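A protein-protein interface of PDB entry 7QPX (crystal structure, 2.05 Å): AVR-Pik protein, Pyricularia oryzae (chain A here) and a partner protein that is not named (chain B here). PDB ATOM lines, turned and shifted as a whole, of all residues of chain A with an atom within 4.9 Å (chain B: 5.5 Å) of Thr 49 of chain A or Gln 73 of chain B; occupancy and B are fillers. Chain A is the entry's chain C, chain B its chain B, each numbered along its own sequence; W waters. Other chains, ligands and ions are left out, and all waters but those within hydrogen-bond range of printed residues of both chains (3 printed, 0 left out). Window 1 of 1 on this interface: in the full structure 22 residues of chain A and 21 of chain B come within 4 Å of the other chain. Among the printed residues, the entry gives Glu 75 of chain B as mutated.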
ATOM      1  N   PHE A  23      14.425  12.522 -30.983  1.00  0.00           N
ATOM      2  CA  PHE A  23      13.026  12.817 -30.578  1.00  0.00           C
ATOM      3  C   PHE A  23      12.339  13.753 -31.581  1.00  0.00           C
ATOM      4  O   PHE A  23      12.986  14.354 -32.421  1.00  0.00           O
ATOM      5  CB  PHE A  23      12.973  13.435 -29.182  1.00  0.00           C
ATOM      6  CG  PHE A  23      13.646  14.781 -29.098  1.00  0.00           C
ATOM      7  CD1 PHE A  23      12.986  15.935 -29.502  1.00  0.00           C
ATOM      8  CD2 PHE A  23      14.953  14.882 -28.648  1.00  0.00           C
ATOM      9  CE1 PHE A  23      13.618  17.168 -29.441  1.00  0.00           C
ATOM     10  CE2 PHE A  23      15.574  16.119 -28.567  1.00  0.00           C
ATOM     11  CZ  PHE A  23      14.906  17.257 -28.965  1.00  0.00           C
ATOM     12  N   ASP A  25       8.959  16.413 -30.827  1.00  0.00           N
ATOM     13  CA  ASP A  25       7.891  16.890 -29.919  1.00  0.00           C
ATOM     14  C   ASP A  25       6.716  17.302 -30.795  1.00  0.00           C
ATOM     15  O   ASP A  25       6.876  18.283 -31.524  1.00  0.00           O
ATOM     16  CB  ASP A  25       8.430  18.006 -29.028  1.00  0.00           C
ATOM     17  CG  ASP A  25       9.515  17.482 -28.102  1.00  0.00           C
ATOM     18  OD1 ASP A  25       9.220  16.541 -27.318  1.00  0.00           O
ATOM     19  OD2 ASP A  25      10.656  17.966 -28.202  1.00  0.00           O
ATOM     20  N   PRO A  32       6.915  16.560 -23.556  1.00  0.00           N
ATOM     21  CA  PRO A  32       7.177  15.622 -22.465  1.00  0.00           C
ATOM     22  C   PRO A  32       8.501  16.003 -21.788  1.00  0.00           C
ATOM     23  O   PRO A  32       9.463  16.295 -22.490  1.00  0.00           O
ATOM     24  CB  PRO A  32       7.228  14.251 -23.168  1.00  0.00           C
ATOM     25  CG  PRO A  32       7.704  14.589 -24.575  1.00  0.00           C
ATOM     26  CD  PRO A  32       7.066  15.934 -24.881  1.00  0.00           C
ATOM     27  N   CYS A  34      10.597  14.166 -19.816  1.00  0.00           N
ATOM     28  CA  CYS A  34      11.599  13.099 -19.529  1.00  0.00           C
ATOM     29  C   CYS A  34      12.140  12.469 -20.816  1.00  0.00           C
ATOM     30  O   CYS A  34      11.389  12.355 -21.808  1.00  0.00           O
ATOM     31  CB  CYS A  34      11.012  11.994 -18.659  1.00  0.00           C
ATOM     32  SG  CYS A  34       9.937  12.599 -17.339  1.00  0.00           S
ATOM     33  N   PHE A  35      13.413  12.089 -20.784  1.00  0.00           N
ATOM     34  CA  PHE A  35      14.030  11.053 -21.646  1.00  0.00           C
ATOM     35  C   PHE A  35      13.913   9.711 -20.912  1.00  0.00           C
ATOM     36  O   PHE A  35      13.855   9.720 -19.656  1.00  0.00           O
ATOM     37  CB  PHE A  35      15.488  11.377 -21.975  1.00  0.00           C
ATOM     38  CG  PHE A  35      15.698  12.523 -22.934  1.00  0.00           C
ATOM     39  CD1 PHE A  35      14.919  12.657 -24.078  1.00  0.00           C
ATOM     40  CD2 PHE A  35      16.709  13.449 -22.716  1.00  0.00           C
ATOM     41  CE1 PHE A  35      15.132  13.699 -24.967  1.00  0.00           C
ATOM     42  CE2 PHE A  35      16.920  14.493 -23.609  1.00  0.00           C
ATOM     43  CZ  PHE A  35      16.137  14.612 -24.733  1.00  0.00           C
ATOM     44  N   TRP A  36      13.786   8.609 -21.658  1.00  0.00           N
ATOM     45  CA  TRP A  36      13.823   7.232 -21.101  1.00  0.00           C
ATOM     46  C   TRP A  36      14.734   6.392 -21.971  1.00  0.00           C
ATOM     47  O   TRP A  36      14.969   6.732 -23.144  1.00  0.00           O
ATOM     48  CB  TRP A  36      12.433   6.603 -20.916  1.00  0.00           C
ATOM     49  CG  TRP A  36      11.649   6.432 -22.185  1.00  0.00           C
ATOM     50  CD1 TRP A  36      10.628   7.216 -22.629  1.00  0.00           C
ATOM     51  CD2 TRP A  36      11.851   5.417 -23.182  1.00  0.00           C
ATOM     52  NE1 TRP A  36      10.177   6.760 -23.842  1.00  0.00           N
ATOM     53  CE2 TRP A  36      10.902   5.654 -24.203  1.00  0.00           C
ATOM     54  CE3 TRP A  36      12.713   4.315 -23.299  1.00  0.00           C
ATOM     55  CZ2 TRP A  36      10.797   4.828 -25.320  1.00  0.00           C
ATOM     56  CZ3 TRP A  36      12.626   3.518 -24.421  1.00  0.00           C
ATOM     57  CH2 TRP A  36      11.671   3.766 -25.410  1.00  0.00           C
ATOM     58  N   ASP A  47      15.183   3.954 -26.822  1.00  0.00           N
ATOM     59  CA  ASP A  47      15.057   5.214 -26.050  1.00  0.00           C
ATOM     60  C   ASP A  47      13.908   6.032 -26.627  1.00  0.00           C
ATOM     61  O   ASP A  47      13.396   5.666 -27.703  1.00  0.00           O
ATOM     62  CB  ASP A  47      16.374   5.995 -26.115  1.00  0.00           C
ATOM     63  CG  ASP A  47      16.892   6.102 -27.537  1.00  0.00           C
ATOM     64  OD1 ASP A  47      16.229   6.775 -28.371  1.00  0.00           O
ATOM     65  OD2 ASP A  47      17.924   5.500 -27.807  1.00  0.00           O
ATOM     66  N   GLY A  48      13.556   7.111 -25.943  1.00  0.00           N
ATOM     67  CA  GLY A  48      12.542   8.069 -26.392  1.00  0.00           C
ATOM     68  C   GLY A  48      12.198   9.015 -25.270  1.00  0.00           C
ATOM     69  O   GLY A  48      13.043   9.189 -24.362  1.00  0.00           O
ATOM     70  N   THR A  49      11.005   9.596 -25.312  1.00  0.00           N
ATOM     71  CA  THR A  49      10.560  10.645 -24.370  1.00  0.00           C
ATOM     72  C   THR A  49       9.282  10.173 -23.698  1.00  0.00           C
ATOM     73  O   THR A  49       8.626   9.275 -24.270  1.00  0.00           O
ATOM     74  CB  THR A  49      10.391  11.979 -25.101  1.00  0.00           C
ATOM     75  OG1 THR A  49       9.404  11.844 -26.120  1.00  0.00           O
ATOM     76  CG2 THR A  49      11.654  12.449 -25.767  1.00  0.00           C
ATOM     77  N   CYS A  50       8.952  10.737 -22.532  1.00  0.00           N
ATOM     78  CA  CYS A  50       7.685  10.477 -21.801  1.00  0.00           C
ATOM     79  C   CYS A  50       7.373  11.634 -20.844  1.00  0.00           C
ATOM     80  O   CYS A  50       8.252  12.435 -20.568  1.00  0.00           O
ATOM     81  CB  CYS A  50       7.748   9.141 -21.060  1.00  0.00           C
ATOM     82  SG  CYS A  50       9.009   9.050 -19.757  1.00  0.00           S
ATOM     83  N   TYR A  51       6.154  11.697 -20.331  1.00  0.00           N
ATOM     84  CA  TYR A  51       5.735  12.772 -19.400  1.00  0.00           C
ATOM     85  C   TYR A  51       6.151  12.423 -17.970  1.00  0.00           C
ATOM     86  O   TYR A  51       6.227  11.227 -17.623  1.00  0.00           O
ATOM     87  CB  TYR A  51       4.238  13.030 -19.483  1.00  0.00           C
ATOM     88  CG  TYR A  51       3.811  13.669 -20.772  1.00  0.00           C
ATOM     89  CD1 TYR A  51       4.077  15.006 -21.035  1.00  0.00           C
ATOM     90  CD2 TYR A  51       3.155  12.925 -21.737  1.00  0.00           C
ATOM     91  CE1 TYR A  51       3.690  15.591 -22.232  1.00  0.00           C
ATOM     92  CE2 TYR A  51       2.747  13.496 -22.929  1.00  0.00           C
ATOM     93  CZ  TYR A  51       3.018  14.829 -23.179  1.00  0.00           C
ATOM     94  OH  TYR A  51       2.590  15.365 -24.359  1.00  0.00           O
ATOM     95  N   MET A  56       2.653   5.385 -18.821  1.00  0.00           N
ATOM     96  CA  MET A  56       2.721   4.906 -20.221  1.00  0.00           C
ATOM     97  C   MET A  56       2.762   3.375 -20.202  1.00  0.00           C
ATOM     98  O   MET A  56       3.082   2.795 -19.130  1.00  0.00           O
ATOM     99  CB  MET A  56       3.963   5.477 -20.901  1.00  0.00           C
ATOM    100  CG  MET A  56       5.258   5.065 -20.242  1.00  0.00           C
ATOM    101  SD  MET A  56       6.622   5.580 -21.244  1.00  0.00           S
ATOM    102  CE  MET A  56       8.006   5.374 -20.121  1.00  0.00           C
ATOM    103  N   ASP A  57       2.427   2.754 -21.336  1.00  0.00           N
ATOM    104  CA  ASP A  57       2.640   1.301 -21.571  1.00  0.00           C
ATOM    105  C   ASP A  57       3.809   1.141 -22.534  1.00  0.00           C
ATOM    106  O   ASP A  57       3.897   1.870 -23.543  1.00  0.00           O
ATOM    107  CB  ASP A  57       1.341   0.623 -22.001  1.00  0.00           C
ATOM    108  CG  ASP A  57       0.258   0.827 -20.950  1.00  0.00           C
ATOM    109  OD1 ASP A  57       0.595   0.900 -19.741  1.00  0.00           O
ATOM    110  OD2 ASP A  57      -0.884   0.914 -21.332  1.00  0.00           O
ATOM    111  N   MET A  58       4.708   0.243 -22.185  1.00  0.00           N
ATOM    112  CA  MET A  58       5.925   0.020 -22.972  1.00  0.00           C
ATOM    113  C   MET A  58       6.101  -1.476 -23.192  1.00  0.00           C
ATOM    114  O   MET A  58       5.904  -2.270 -22.231  1.00  0.00           O
ATOM    115  CB  MET A  58       7.148   0.582 -22.253  1.00  0.00           C
ATOM    116  CG  MET A  58       8.362   0.561 -23.144  1.00  0.00           C
ATOM    117  SD  MET A  58       9.731   1.569 -22.535  1.00  0.00           S
ATOM    118  CE  MET A  58       9.050   3.207 -22.742  1.00  0.00           C
ATOM    119  N   TRP A  64       4.356  -6.277 -22.173  1.00  0.00           N
ATOM    120  CA  TRP A  64       3.778  -4.939 -21.896  1.00  0.00           C
ATOM    121  C   TRP A  64       3.938  -4.618 -20.415  1.00  0.00           C
ATOM    122  O   TRP A  64       3.537  -5.440 -19.562  1.00  0.00           O
ATOM    123  CB  TRP A  64       2.321  -4.888 -22.337  1.00  0.00           C
ATOM    124  CG  TRP A  64       2.244  -4.692 -23.815  1.00  0.00           C
ATOM    125  CD1 TRP A  64       1.975  -5.634 -24.770  1.00  0.00           C
ATOM    126  CD2 TRP A  64       2.553  -3.474 -24.515  1.00  0.00           C
ATOM    127  NE1 TRP A  64       2.034  -5.066 -26.019  1.00  0.00           N
ATOM    128  CE2 TRP A  64       2.393  -3.742 -25.892  1.00  0.00           C
ATOM    129  CE3 TRP A  64       2.944  -2.191 -24.117  1.00  0.00           C
ATOM    130  CZ2 TRP A  64       2.589  -2.756 -26.860  1.00  0.00           C
ATOM    131  CZ3 TRP A  64       3.141  -1.220 -25.076  1.00  0.00           C
ATOM    132  CH2 TRP A  64       2.974  -1.506 -26.429  1.00  0.00           C
ATOM    133  N   ARG A  90      14.780  16.132 -19.251  1.00  0.00           N
ATOM    134  CA  ARG A  90      15.451  16.643 -20.472  1.00  0.00           C
ATOM    135  C   ARG A  90      16.059  18.004 -20.128  1.00  0.00           C
ATOM    136  O   ARG A  90      15.596  18.647 -19.185  1.00  0.00           O
ATOM    137  CB  ARG A  90      14.429  16.776 -21.609  1.00  0.00           C
ATOM    138  CG  ARG A  90      13.699  15.486 -21.971  1.00  0.00           C
ATOM    139  CD  ARG A  90      12.502  15.812 -22.830  1.00  0.00           C
ATOM    140  NE  ARG A  90      12.912  16.292 -24.141  1.00  0.00           N
ATOM    141  CZ  ARG A  90      12.070  16.571 -25.134  1.00  0.00           C
ATOM    142  NH1 ARG A  90      10.760  16.449 -24.953  1.00  0.00           N
ATOM    143  NH2 ARG A  90      12.552  16.954 -26.306  1.00  0.00           N
ATOM    144  N   LYS B   7       0.004   9.284 -27.909  1.00  0.00           N
ATOM    145  CA  LYS B   7       1.273   9.063 -28.619  1.00  0.00           C
ATOM    146  C   LYS B   7       1.500   7.556 -28.695  1.00  0.00           C
ATOM    147  O   LYS B   7       1.379   6.884 -27.631  1.00  0.00           O
ATOM    148  CB  LYS B   7       2.398   9.755 -27.851  1.00  0.00           C
ATOM    149  CG  LYS B   7       3.811   9.493 -28.345  1.00  0.00           C
ATOM    150  CD  LYS B   7       4.825  10.217 -27.466  1.00  0.00           C
ATOM    151  CE  LYS B   7       6.135   9.482 -27.349  1.00  0.00           C
ATOM    152  NZ  LYS B   7       7.197  10.373 -26.836  1.00  0.00           N
ATOM    153  N   ILE B   8       1.851   7.092 -29.887  1.00  0.00           N
ATOM    154  CA  ILE B   8       2.142   5.672 -30.214  1.00  0.00           C
ATOM    155  C   ILE B   8       3.522   5.645 -30.856  1.00  0.00           C
ATOM    156  O   ILE B   8       3.740   6.419 -31.804  1.00  0.00           O
ATOM    157  CB  ILE B   8       1.077   5.128 -31.186  1.00  0.00           C
ATOM    158  CG1 ILE B   8      -0.309   5.064 -30.542  1.00  0.00           C
ATOM    159  CG2 ILE B   8       1.470   3.777 -31.762  1.00  0.00           C
ATOM    160  CD1 ILE B   8      -1.394   4.811 -31.567  1.00  0.00           C
ATOM    161  N   VAL B   9       4.407   4.771 -30.409  1.00  0.00           N
ATOM    162  CA  VAL B   9       5.711   4.583 -31.088  1.00  0.00           C
ATOM    163  C   VAL B   9       5.754   3.157 -31.629  1.00  0.00           C
ATOM    164  O   VAL B   9       5.469   2.230 -30.859  1.00  0.00           O
ATOM    165  CB  VAL B   9       6.897   4.891 -30.163  1.00  0.00           C
ATOM    166  CG1 VAL B   9       8.233   4.746 -30.888  1.00  0.00           C
ATOM    167  CG2 VAL B   9       6.786   6.273 -29.556  1.00  0.00           C
ATOM    168  N   GLU B  47       6.687   7.617 -34.814  1.00  0.00           N
ATOM    169  CA  GLU B  47       5.952   8.188 -33.666  1.00  0.00           C
ATOM    170  C   GLU B  47       4.719   8.903 -34.213  1.00  0.00           C
ATOM    171  O   GLU B  47       4.886   9.774 -35.089  1.00  0.00           O
ATOM    172  CB  GLU B  47       6.875   9.113 -32.893  1.00  0.00           C
ATOM    173  CG  GLU B  47       6.183   9.721 -31.707  1.00  0.00           C
ATOM    174  CD  GLU B  47       7.162  10.413 -30.787  1.00  0.00           C
ATOM    175  OE1 GLU B  47       6.728  11.363 -30.112  1.00  0.00           O
ATOM    176  OE2 GLU B  47       8.342   9.974 -30.748  1.00  0.00           O
ATOM    177  N   LEU B  71       4.552  -2.551 -31.779  1.00  0.00           N
ATOM    178  CA  LEU B  71       4.259  -1.447 -30.823  1.00  0.00           C
ATOM    179  C   LEU B  71       5.372  -1.366 -29.759  1.00  0.00           C
ATOM    180  O   LEU B  71       5.628  -2.402 -29.134  1.00  0.00           O
ATOM    181  CB  LEU B  71       2.918  -1.730 -30.147  1.00  0.00           C
ATOM    182  CG  LEU B  71       1.682  -1.253 -30.879  1.00  0.00           C
ATOM    183  CD1 LEU B  71       0.431  -1.773 -30.193  1.00  0.00           C
ATOM    184  CD2 LEU B  71       1.665   0.262 -30.960  1.00  0.00           C
ATOM    185  N   LEU B  72       5.942  -0.169 -29.508  1.00  0.00           N
ATOM    186  CA  LEU B  72       6.978   0.065 -28.460  1.00  0.00           C
ATOM    187  C   LEU B  72       6.384   0.811 -27.259  1.00  0.00           C
ATOM    188  O   LEU B  72       6.619   0.369 -26.140  1.00  0.00           O
ATOM    189  CB  LEU B  72       8.155   0.847 -29.050  1.00  0.00           C
ATOM    190  CG  LEU B  72       9.311   1.139 -28.081  1.00  0.00           C
ATOM    191  CD1 LEU B  72       9.831  -0.118 -27.417  1.00  0.00           C
ATOM    192  CD2 LEU B  72      10.448   1.843 -28.792  1.00  0.00           C
ATOM    193  N   GLN B  73       5.674   1.910 -27.500  1.00  0.00           N
ATOM    194  CA  GLN B  73       5.223   2.841 -26.441  1.00  0.00           C
ATOM    195  C   GLN B  73       3.833   3.365 -26.809  1.00  0.00           C
ATOM    196  O   GLN B  73       3.574   3.743 -27.991  1.00  0.00           O
ATOM    197  CB  GLN B  73       6.240   3.970 -26.261  1.00  0.00           C
ATOM    198  CG  GLN B  73       5.866   5.019 -25.211  1.00  0.00           C
ATOM    199  CD  GLN B  73       6.806   6.210 -25.214  1.00  0.00           C
ATOM    200  OE1 GLN B  73       7.811   6.225 -25.911  1.00  0.00           O
ATOM    201  NE2 GLN B  73       6.472   7.242 -24.454  1.00  0.00           N
ATOM    202  N   VAL B  74       2.957   3.372 -25.820  1.00  0.00           N
ATOM    203  CA  VAL B  74       1.631   4.030 -25.893  1.00  0.00           C
ATOM    204  C   VAL B  74       1.488   4.876 -24.642  1.00  0.00           C
ATOM    205  O   VAL B  74       1.624   4.308 -23.516  1.00  0.00           O
ATOM    206  CB  VAL B  74       0.481   3.021 -26.005  1.00  0.00           C
ATOM    207  CG1 VAL B  74      -0.853   3.748 -26.131  1.00  0.00           C
ATOM    208  CG2 VAL B  74       0.705   2.097 -27.198  1.00  0.00           C
ATOM    209  N   GLU B  75       1.241   6.167 -24.850  1.00  0.00           N
ATOM    210  CA  GLU B  75       1.127   7.154 -23.753  1.00  0.00           C
ATOM    211  C   GLU B  75       0.055   8.184 -24.098  1.00  0.00           C
ATOM    212  O   GLU B  75       0.156   8.786 -25.196  1.00  0.00           O
ATOM    213  CB  GLU B  75       2.458   7.853 -23.543  1.00  0.00           C
ATOM    214  CG  GLU B  75       2.467   8.761 -22.323  1.00  0.00           C
ATOM    215  CD  GLU B  75       3.834   9.391 -22.174  1.00  0.00           C
ATOM    216  OE1 GLU B  75       4.589   9.397 -23.187  1.00  0.00           O
ATOM    217  OE2 GLU B  75       4.165   9.842 -21.065  1.00  0.00           O
HETATM  218  O   HOH W   1       5.065   8.922 -18.685  1.00  0.00           O
HETATM  219  O   HOH W   2       7.004  13.017 -28.237  1.00  0.00           O
HETATM  220  O   HOH W   3       9.195   8.196 -27.097  1.00  0.00           O
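NE1 of Trp 36 of chain A lies within hydrogen-bond range of O of Thr 49 of chain A.
The backbone carbonyl oxygen of Val 9 of chain B lies within hydrogen-bond range of the backbone NH of Leu 72 of chain B (2.8 Å).
N of Cys 34 of chain A is in hydrogen-bond range of O of Cys 50 of chain A (3.0 Å).
The backbone NH (N) of Trp 36 of chain A is in hydrogen-bond range of the backbone carbonyl oxygen (O) of Gly 48 of chain A.
The side-chain carboxylate of Glu 47 of chain B is in salt-bridge range of the side-chain amino group of Lys 7 of chain B (3.5 Å).
OE1 of Glu 75 of chain B is in hydrogen-bond range of NE2 of Gln 73 of chain B, at 3.1 Å.
Water W2 lies within hydrogen-bond range of OE1 of Glu 47 of chain B, NZ of Lys 7 of chain B and OG1 of Thr 49 of chain A.
Water W3 lies within hydrogen-bond range of OE1 of Gln 73 of chain B, N of Thr 49 of chain A and NZ of Lys 7 of chain B.
Water W1 bridges the side-chain carboxylate (OE2) of Glu 75 of chain B (2.7 Å) and the backbone carbonyl oxygen (O) of Tyr 51 of chain A (2.8 Å).
Of the 9 printed residues of chain B, 6 touch a printed residue of chain A.
Hydrophobic or aromatic side chains of chain B that line the printed part of chain A: Leu 71.
Among the printed residues, 13 pairs touch across the chains.
Among the printed residues, no Asp or Glu carboxylate lies within 4 Å of a Lys or Arg side-chain nitrogen of the other chain.
Glu 75 of chain B touches Cys 50 of chain A (OE1 to CA, 3.6 Å).
O of Val 74 of chain B touches CA of Met 56 of chain A, at 3.5 Å.
Met 56 of chain A touches Glu 75 of chain B.
Asp 57 of chain A touches Gln 73 of chain B.
CA of Met 58 of chain A touches O of Leu 72 of chain B (3.3 Å).
Leu 71 of chain B touches Trp 64 of chain A (CB to CZ2, 3.5 Å).
Leu 72 of chain B touches Trp 64 of chain A (O to CZ3, 3.97 Å).
Asp 25 of chain A touches none of the printed residues of chain B.
Thr 49 of chain A touches two residues of chain B.
Of the printed residues of chain B, Met 56 of chain A touches Gln 73 (3.6 Å), Val 74 (3.5 Å) and Glu 75 (3.9 Å).
Of the printed residues of chain A, Lys 7 of chain B touches Thr 49.
Gln 73 of chain B touches four residues of chain A.
Of the printed residues of chain A, Val 74 of chain B touches Met 56 and Asp 57.
The nearest residue of chain B that does not touch Thr 49 of chain A is Glu 75 of chain B (4.2 Å).
The nearest printed residue of chain B that does not touch Met 56 of chain A is Leu 72 of chain B (7.2 Å).
OE1 of Gln 73 of chain B is in hydrogen-bond range of NE1 of Trp 36 of chain A (3.2 Å).
NE2 of Gln 73 of chain B sits at hydrogen-bond distance from O of Thr 49 of chain A, at 3.0 Å.
SD of Met 56 of chain A lies within hydrogen-bond range of NE2 of Gln 73 of chain B.
The backbone NH (N) of Tyr 51 of chain A sits at hydrogen-bond distance from the side-chain carboxylate (OE2) of Glu 75 of chain B.
The side-chain hydroxyl (OG1) of Thr 49 of chain A lies within hydrogen-bond range of the side-chain amino group (NZ) of Lys 7 of chain B (2.7 Å).
The backbone NH of Asp 57 of chain A sits at hydrogen-bond distance from the backbone carbonyl oxygen of Val 74 of chain B, 2.8 Å away.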
